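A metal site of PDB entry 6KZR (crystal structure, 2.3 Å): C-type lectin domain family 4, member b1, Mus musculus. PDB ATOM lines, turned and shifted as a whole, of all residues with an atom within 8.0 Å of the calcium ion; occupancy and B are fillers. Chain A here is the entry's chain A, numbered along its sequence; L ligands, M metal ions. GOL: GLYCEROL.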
ATOM      1  N   ARG A  74      24.615 -16.085  -1.379  1.00  0.00           N
ATOM      2  CA  ARG A  74      23.359 -16.869  -1.433  1.00  0.00           C
ATOM      3  C   ARG A  74      22.471 -16.454  -0.260  1.00  0.00           C
ATOM      4  O   ARG A  74      21.772 -17.323   0.268  1.00  0.00           O
ATOM      5  CB  ARG A  74      23.646 -18.372  -1.394  1.00  0.00           C
ATOM      6  CG  ARG A  74      24.840 -18.825  -2.236  1.00  0.00           C
ATOM      7  CD  ARG A  74      24.625 -18.732  -3.728  1.00  0.00           C
ATOM      8  NE  ARG A  74      24.712 -17.371  -4.248  1.00  0.00           N
ATOM      9  CZ  ARG A  74      24.468 -17.031  -5.513  1.00  0.00           C
ATOM     10  NH1 ARG A  74      24.548 -15.758  -5.883  1.00  0.00           N
ATOM     11  NH2 ARG A  74      24.153 -17.954  -6.404  1.00  0.00           N
ATOM     12  N   TRP A  76      19.528 -14.659  -0.053  1.00  0.00           N
ATOM     13  CA  TRP A  76      18.417 -14.170  -0.909  1.00  0.00           C
ATOM     14  C   TRP A  76      17.467 -13.313  -0.053  1.00  0.00           C
ATOM     15  O   TRP A  76      17.185 -13.694   1.092  1.00  0.00           O
ATOM     16  CB  TRP A  76      17.730 -15.356  -1.561  1.00  0.00           C
ATOM     17  CG  TRP A  76      18.680 -16.190  -2.360  1.00  0.00           C
ATOM     18  CD1 TRP A  76      19.170 -17.423  -2.048  1.00  0.00           C
ATOM     19  CD2 TRP A  76      19.314 -15.802  -3.593  1.00  0.00           C
ATOM     20  NE1 TRP A  76      20.035 -17.839  -3.023  1.00  0.00           N
ATOM     21  CE2 TRP A  76      20.151 -16.863  -3.970  1.00  0.00           C
ATOM     22  CE3 TRP A  76      19.243 -14.672  -4.402  1.00  0.00           C
ATOM     23  CZ2 TRP A  76      20.918 -16.820  -5.130  1.00  0.00           C
ATOM     24  CZ3 TRP A  76      20.003 -14.629  -5.549  1.00  0.00           C
ATOM     25  CH2 TRP A  76      20.824 -15.695  -5.910  1.00  0.00           C
ATOM     26  N   TRP A  91      13.666 -22.770  -7.813  1.00  0.00           N
ATOM     27  CA  TRP A  91      14.932 -22.782  -8.593  1.00  0.00           C
ATOM     28  C   TRP A  91      14.861 -23.900  -9.631  1.00  0.00           C
ATOM     29  O   TRP A  91      14.448 -25.002  -9.260  1.00  0.00           O
ATOM     30  CB  TRP A  91      16.156 -22.975  -7.683  1.00  0.00           C
ATOM     31  CG  TRP A  91      16.336 -21.889  -6.665  1.00  0.00           C
ATOM     32  CD1 TRP A  91      16.051 -21.965  -5.328  1.00  0.00           C
ATOM     33  CD2 TRP A  91      16.822 -20.564  -6.891  1.00  0.00           C
ATOM     34  NE1 TRP A  91      16.342 -20.767  -4.717  1.00  0.00           N
ATOM     35  CE2 TRP A  91      16.819 -19.898  -5.658  1.00  0.00           C
ATOM     36  CE3 TRP A  91      17.288 -19.891  -8.024  1.00  0.00           C
ATOM     37  CZ2 TRP A  91      17.256 -18.588  -5.516  1.00  0.00           C
ATOM     38  CZ3 TRP A  91      17.700 -18.591  -7.896  1.00  0.00           C
ATOM     39  CH2 TRP A  91      17.693 -17.950  -6.649  1.00  0.00           C
ATOM     40  N   GLY A  94      20.143 -27.300 -10.984  1.00  0.00           N
ATOM     41  CA  GLY A  94      21.476 -26.675 -11.130  1.00  0.00           C
ATOM     42  C   GLY A  94      21.481 -25.179 -10.774  1.00  0.00           C
ATOM     43  O   GLY A  94      22.541 -24.540 -10.958  1.00  0.00           O
ATOM     44  N   GLU A  95      20.363 -24.616 -10.310  1.00  0.00           N
ATOM     45  CA  GLU A  95      20.297 -23.196  -9.880  1.00  0.00           C
ATOM     46  C   GLU A  95      19.980 -23.140  -8.391  1.00  0.00           C
ATOM     47  O   GLU A  95      19.316 -24.018  -7.852  1.00  0.00           O
ATOM     48  CB  GLU A  95      19.258 -22.381 -10.657  1.00  0.00           C
ATOM     49  CG  GLU A  95      19.429 -22.438 -12.169  1.00  0.00           C
ATOM     50  CD  GLU A  95      20.753 -21.930 -12.731  1.00  0.00           C
ATOM     51  OE1 GLU A  95      21.464 -21.194 -12.026  1.00  0.00           O
ATOM     52  OE2 GLU A  95      21.052 -22.262 -13.899  1.00  0.00           O
ATOM     53  N   PRO A  96      20.471 -22.111  -7.662  1.00  0.00           N
ATOM     54  CA  PRO A  96      21.413 -21.114  -8.201  1.00  0.00           C
ATOM     55  C   PRO A  96      22.785 -21.688  -8.583  1.00  0.00           C
ATOM     56  O   PRO A  96      23.141 -22.692  -8.053  1.00  0.00           O
ATOM     57  CB  PRO A  96      21.638 -20.144  -7.037  1.00  0.00           C
ATOM     58  CG  PRO A  96      20.476 -20.386  -6.103  1.00  0.00           C
ATOM     59  CD  PRO A  96      20.109 -21.839  -6.271  1.00  0.00           C
ATOM     60  N   SER A  97      23.523 -20.997  -9.444  1.00  0.00           N
ATOM     61  CA  SER A  97      24.699 -21.556 -10.159  1.00  0.00           C
ATOM     62  C   SER A  97      25.995 -20.799  -9.834  1.00  0.00           C
ATOM     63  O   SER A  97      27.041 -21.444  -9.982  1.00  0.00           O
ATOM     64  CB  SER A  97      24.462 -21.566 -11.639  1.00  0.00           C
ATOM     65  OG  SER A  97      24.289 -20.244 -12.124  1.00  0.00           O
ATOM     66  N   SER A  98      25.942 -19.510  -9.485  1.00  0.00           N
ATOM     67  CA  SER A  98      27.171 -18.660  -9.382  1.00  0.00           C
ATOM     68  C   SER A  98      26.993 -17.513  -8.391  1.00  0.00           C
ATOM     69  O   SER A  98      26.010 -16.738  -8.515  1.00  0.00           O
ATOM     70  CB  SER A  98      27.564 -18.131 -10.724  1.00  0.00           C
ATOM     71  OG  SER A  98      28.435 -17.024 -10.593  1.00  0.00           O
ATOM     72  N   ASP A  99      27.962 -17.336  -7.494  1.00  0.00           N
ATOM     73  CA  ASP A  99      27.957 -16.270  -6.473  1.00  0.00           C
ATOM     74  C   ASP A  99      28.148 -14.904  -7.136  1.00  0.00           C
ATOM     75  O   ASP A  99      27.925 -13.896  -6.453  1.00  0.00           O
ATOM     76  CB  ASP A  99      28.998 -16.507  -5.365  1.00  0.00           C
ATOM     77  CG  ASP A  99      28.670 -15.741  -4.093  1.00  0.00           C
ATOM     78  OD1 ASP A  99      27.463 -15.691  -3.742  1.00  0.00           O
ATOM     79  OD2 ASP A  99      29.611 -15.169  -3.470  1.00  0.00           O
ATOM     80  N   GLU A 101      26.240 -14.132  -9.741  1.00  0.00           N
ATOM     81  CA  GLU A 101      24.862 -13.837 -10.227  1.00  0.00           C
ATOM     82  C   GLU A 101      23.988 -13.428  -9.030  1.00  0.00           C
ATOM     83  O   GLU A 101      23.641 -14.313  -8.235  1.00  0.00           O
ATOM     84  CB  GLU A 101      24.340 -15.044 -11.005  1.00  0.00           C
ATOM     85  CG  GLU A 101      25.175 -15.357 -12.248  1.00  0.00           C
ATOM     86  CD  GLU A 101      24.681 -16.523 -13.076  1.00  0.00           C
ATOM     87  OE1 GLU A 101      24.237 -17.530 -12.488  1.00  0.00           O
ATOM     88  OE2 GLU A 101      24.715 -16.415 -14.326  1.00  0.00           O
ATOM     89  N   CYS A 103      21.033 -11.457  -8.983  1.00  0.00           N
ATOM     90  CA  CYS A 103      19.620 -11.152  -9.287  1.00  0.00           C
ATOM     91  C   CYS A 103      18.934 -12.418  -9.816  1.00  0.00           C
ATOM     92  O   CYS A 103      19.643 -13.366 -10.167  1.00  0.00           O
ATOM     93  CB  CYS A 103      19.528  -9.991 -10.268  1.00  0.00           C
ATOM     94  SG  CYS A 103      19.894  -8.431  -9.438  1.00  0.00           S
ATOM     95  N   THR A 105      15.847 -14.314 -12.203  1.00  0.00           N
ATOM     96  CA  THR A 105      14.936 -14.315 -13.351  1.00  0.00           C
ATOM     97  C   THR A 105      14.077 -15.577 -13.242  1.00  0.00           C
ATOM     98  O   THR A 105      14.524 -16.542 -12.598  1.00  0.00           O
ATOM     99  CB  THR A 105      15.789 -14.196 -14.610  1.00  0.00           C
ATOM    100  OG1 THR A 105      14.987 -13.529 -15.570  1.00  0.00           O
ATOM    101  CG2 THR A 105      16.274 -15.536 -15.107  1.00  0.00           C
ATOM    102  N   TYR A 107      12.071 -18.200 -15.944  1.00  0.00           N
ATOM    103  CA  TYR A 107      11.993 -18.564 -17.383  1.00  0.00           C
ATOM    104  C   TYR A 107      11.548 -20.018 -17.505  1.00  0.00           C
ATOM    105  O   TYR A 107      11.608 -20.813 -16.542  1.00  0.00           O
ATOM    106  CB  TYR A 107      13.309 -18.244 -18.095  1.00  0.00           C
ATOM    107  CG  TYR A 107      14.340 -19.333 -18.074  1.00  0.00           C
ATOM    108  CD1 TYR A 107      15.141 -19.541 -16.970  1.00  0.00           C
ATOM    109  CD2 TYR A 107      14.547 -20.146 -19.178  1.00  0.00           C
ATOM    110  CE1 TYR A 107      16.120 -20.531 -16.937  1.00  0.00           C
ATOM    111  CE2 TYR A 107      15.519 -21.138 -19.165  1.00  0.00           C
ATOM    112  CZ  TYR A 107      16.308 -21.334 -18.043  1.00  0.00           C
ATOM    113  OH  TYR A 107      17.270 -22.299 -18.044  1.00  0.00           O
ATOM    114  N   ARG A 109      11.860 -23.708 -19.193  1.00  0.00           N
ATOM    115  CA  ARG A 109      12.701 -24.737 -19.850  1.00  0.00           C
ATOM    116  C   ARG A 109      11.777 -25.730 -20.560  1.00  0.00           C
ATOM    117  O   ARG A 109      10.901 -26.295 -19.872  1.00  0.00           O
ATOM    118  CB  ARG A 109      13.550 -25.499 -18.824  1.00  0.00           C
ATOM    119  CG  ARG A 109      14.824 -24.790 -18.413  1.00  0.00           C
ATOM    120  CD  ARG A 109      15.602 -25.646 -17.417  1.00  0.00           C
ATOM    121  NE  ARG A 109      16.844 -25.021 -16.991  1.00  0.00           N
ATOM    122  CZ  ARG A 109      17.672 -25.489 -16.049  1.00  0.00           C
ATOM    123  NH1 ARG A 109      18.782 -24.821 -15.752  1.00  0.00           N
ATOM    124  NH2 ARG A 109      17.394 -26.610 -15.401  1.00  0.00           N
ATOM    125  N   TRP A 116      13.268 -20.626 -11.444  1.00  0.00           N
ATOM    126  CA  TRP A 116      14.142 -19.456 -11.198  1.00  0.00           C
ATOM    127  C   TRP A 116      15.567 -19.755 -11.687  1.00  0.00           C
ATOM    128  O   TRP A 116      15.998 -20.919 -11.609  1.00  0.00           O
ATOM    129  CB  TRP A 116      14.129 -19.083  -9.728  1.00  0.00           C
ATOM    130  CG  TRP A 116      12.781 -18.765  -9.179  1.00  0.00           C
ATOM    131  CD1 TRP A 116      11.609 -18.534  -9.843  1.00  0.00           C
ATOM    132  CD2 TRP A 116      12.479 -18.589  -7.780  1.00  0.00           C
ATOM    133  NE1 TRP A 116      10.602 -18.263  -8.953  1.00  0.00           N
ATOM    134  CE2 TRP A 116      11.111 -18.268  -7.687  1.00  0.00           C
ATOM    135  CE3 TRP A 116      13.252 -18.662  -6.618  1.00  0.00           C
ATOM    136  CZ2 TRP A 116      10.495 -18.047  -6.460  1.00  0.00           C
ATOM    137  CZ3 TRP A 116      12.629 -18.439  -5.404  1.00  0.00           C
ATOM    138  CH2 TRP A 116      11.279 -18.129  -5.341  1.00  0.00           C
ATOM    139  N   ASN A 117      16.248 -18.708 -12.137  1.00  0.00           N
ATOM    140  CA  ASN A 117      17.698 -18.739 -12.475  1.00  0.00           C
ATOM    141  C   ASN A 117      18.371 -17.507 -11.880  1.00  0.00           C
ATOM    142  O   ASN A 117      17.867 -16.400 -12.055  1.00  0.00           O
ATOM    143  CB  ASN A 117      17.916 -18.783 -13.978  1.00  0.00           C
ATOM    144  CG  ASN A 117      19.388 -18.740 -14.337  1.00  0.00           C
ATOM    145  OD1 ASN A 117      20.218 -19.268 -13.604  1.00  0.00           O
ATOM    146  ND2 ASN A 117      19.690 -18.092 -15.456  1.00  0.00           N
ATOM    147  N   ASP A 118      19.510 -17.688 -11.227  1.00  0.00           N
ATOM    148  CA  ASP A 118      20.323 -16.526 -10.797  1.00  0.00           C
ATOM    149  C   ASP A 118      21.077 -16.050 -12.037  1.00  0.00           C
ATOM    150  O   ASP A 118      21.568 -16.903 -12.806  1.00  0.00           O
ATOM    151  CB  ASP A 118      21.179 -16.867  -9.573  1.00  0.00           C
ATOM    152  CG  ASP A 118      22.254 -17.916  -9.818  1.00  0.00           C
ATOM    153  OD1 ASP A 118      22.026 -18.809 -10.669  1.00  0.00           O
ATOM    154  OD2 ASP A 118      23.296 -17.834  -9.154  1.00  0.00           O
ATOM    155  N   ILE A 119      21.069 -14.730 -12.293  1.00  0.00           N
ATOM    156  CA  ILE A 119      21.830 -14.103 -13.409  1.00  0.00           C
ATOM    157  C   ILE A 119      22.438 -12.782 -12.955  1.00  0.00           C
ATOM    158  O   ILE A 119      22.083 -12.290 -11.875  1.00  0.00           O
ATOM    159  CB  ILE A 119      20.967 -13.858 -14.661  1.00  0.00           C
ATOM    160  CG1 ILE A 119      19.796 -12.930 -14.371  1.00  0.00           C
ATOM    161  CG2 ILE A 119      20.518 -15.150 -15.302  1.00  0.00           C
ATOM    162  CD1 ILE A 119      19.226 -12.319 -15.631  1.00  0.00           C
ATOM    163  N   SER A 120      23.318 -12.248 -13.786  1.00  0.00           N
ATOM    164  CA  SER A 120      23.894 -10.889 -13.656  1.00  0.00           C
ATOM    165  C   SER A 120      22.753  -9.856 -13.609  1.00  0.00           C
ATOM    166  O   SER A 120      21.867  -9.879 -14.510  1.00  0.00           O
ATOM    167  CB  SER A 120      24.872 -10.604 -14.781  1.00  0.00           C
ATOM    168  OG  SER A 120      24.998  -9.215 -14.956  1.00  0.00           O
HETATM  169  C1  GOL L   1      23.110 -20.379 -16.085  1.00  0.00           C
HETATM  170  O1  GOL L   1      22.873 -20.850 -14.762  1.00  0.00           O
HETATM  171  C2  GOL L   1      22.674 -18.947 -16.215  1.00  0.00           C
HETATM  172  O2  GOL L   1      23.311 -18.119 -15.251  1.00  0.00           O
HETATM  173  C3  GOL L   1      22.894 -18.378 -17.588  1.00  0.00           C
HETATM  174  O3  GOL L   1      21.766 -17.595 -17.969  1.00  0.00           O
HETATM  175 CA    CA M   1      22.451 -19.059 -12.938  1.00  0.00          CA
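The calcium ion is bound by OD1 of Asp 118 (2.3 Å), O of Asp 118 (2.3 Å), OG of Ser 97 (2.3 Å), OD1 of Asn 117 (2.3 Å), OE1 of Glu 101 (2.4 Å), OE1 of Glu 95 (2.5 Å), O1 of the ligand (2.6 Å) and O2 of the ligand (2.6 Å).
OD2 of Asp 118 sits at hydrogen-bond distance from N of Ser 98 (3.1 Å).
OD2 of Asp 118 is in salt-bridge range of NH2 of Arg 74, 2.9 Å away.
O of Thr 105 is in hydrogen-bond range of N of Asn 117 (2.8 Å).
NH1 of Arg 74 sits at hydrogen-bond distance from O of Glu 101, at 2.9 Å.
The side-chain carboxylate of Glu 95 is in salt-bridge range of the guanidinium group of Arg 109 (3.9 Å).
The nearest printed residue that does not touch the calcium ion is Ile 119 (4.6 Å).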
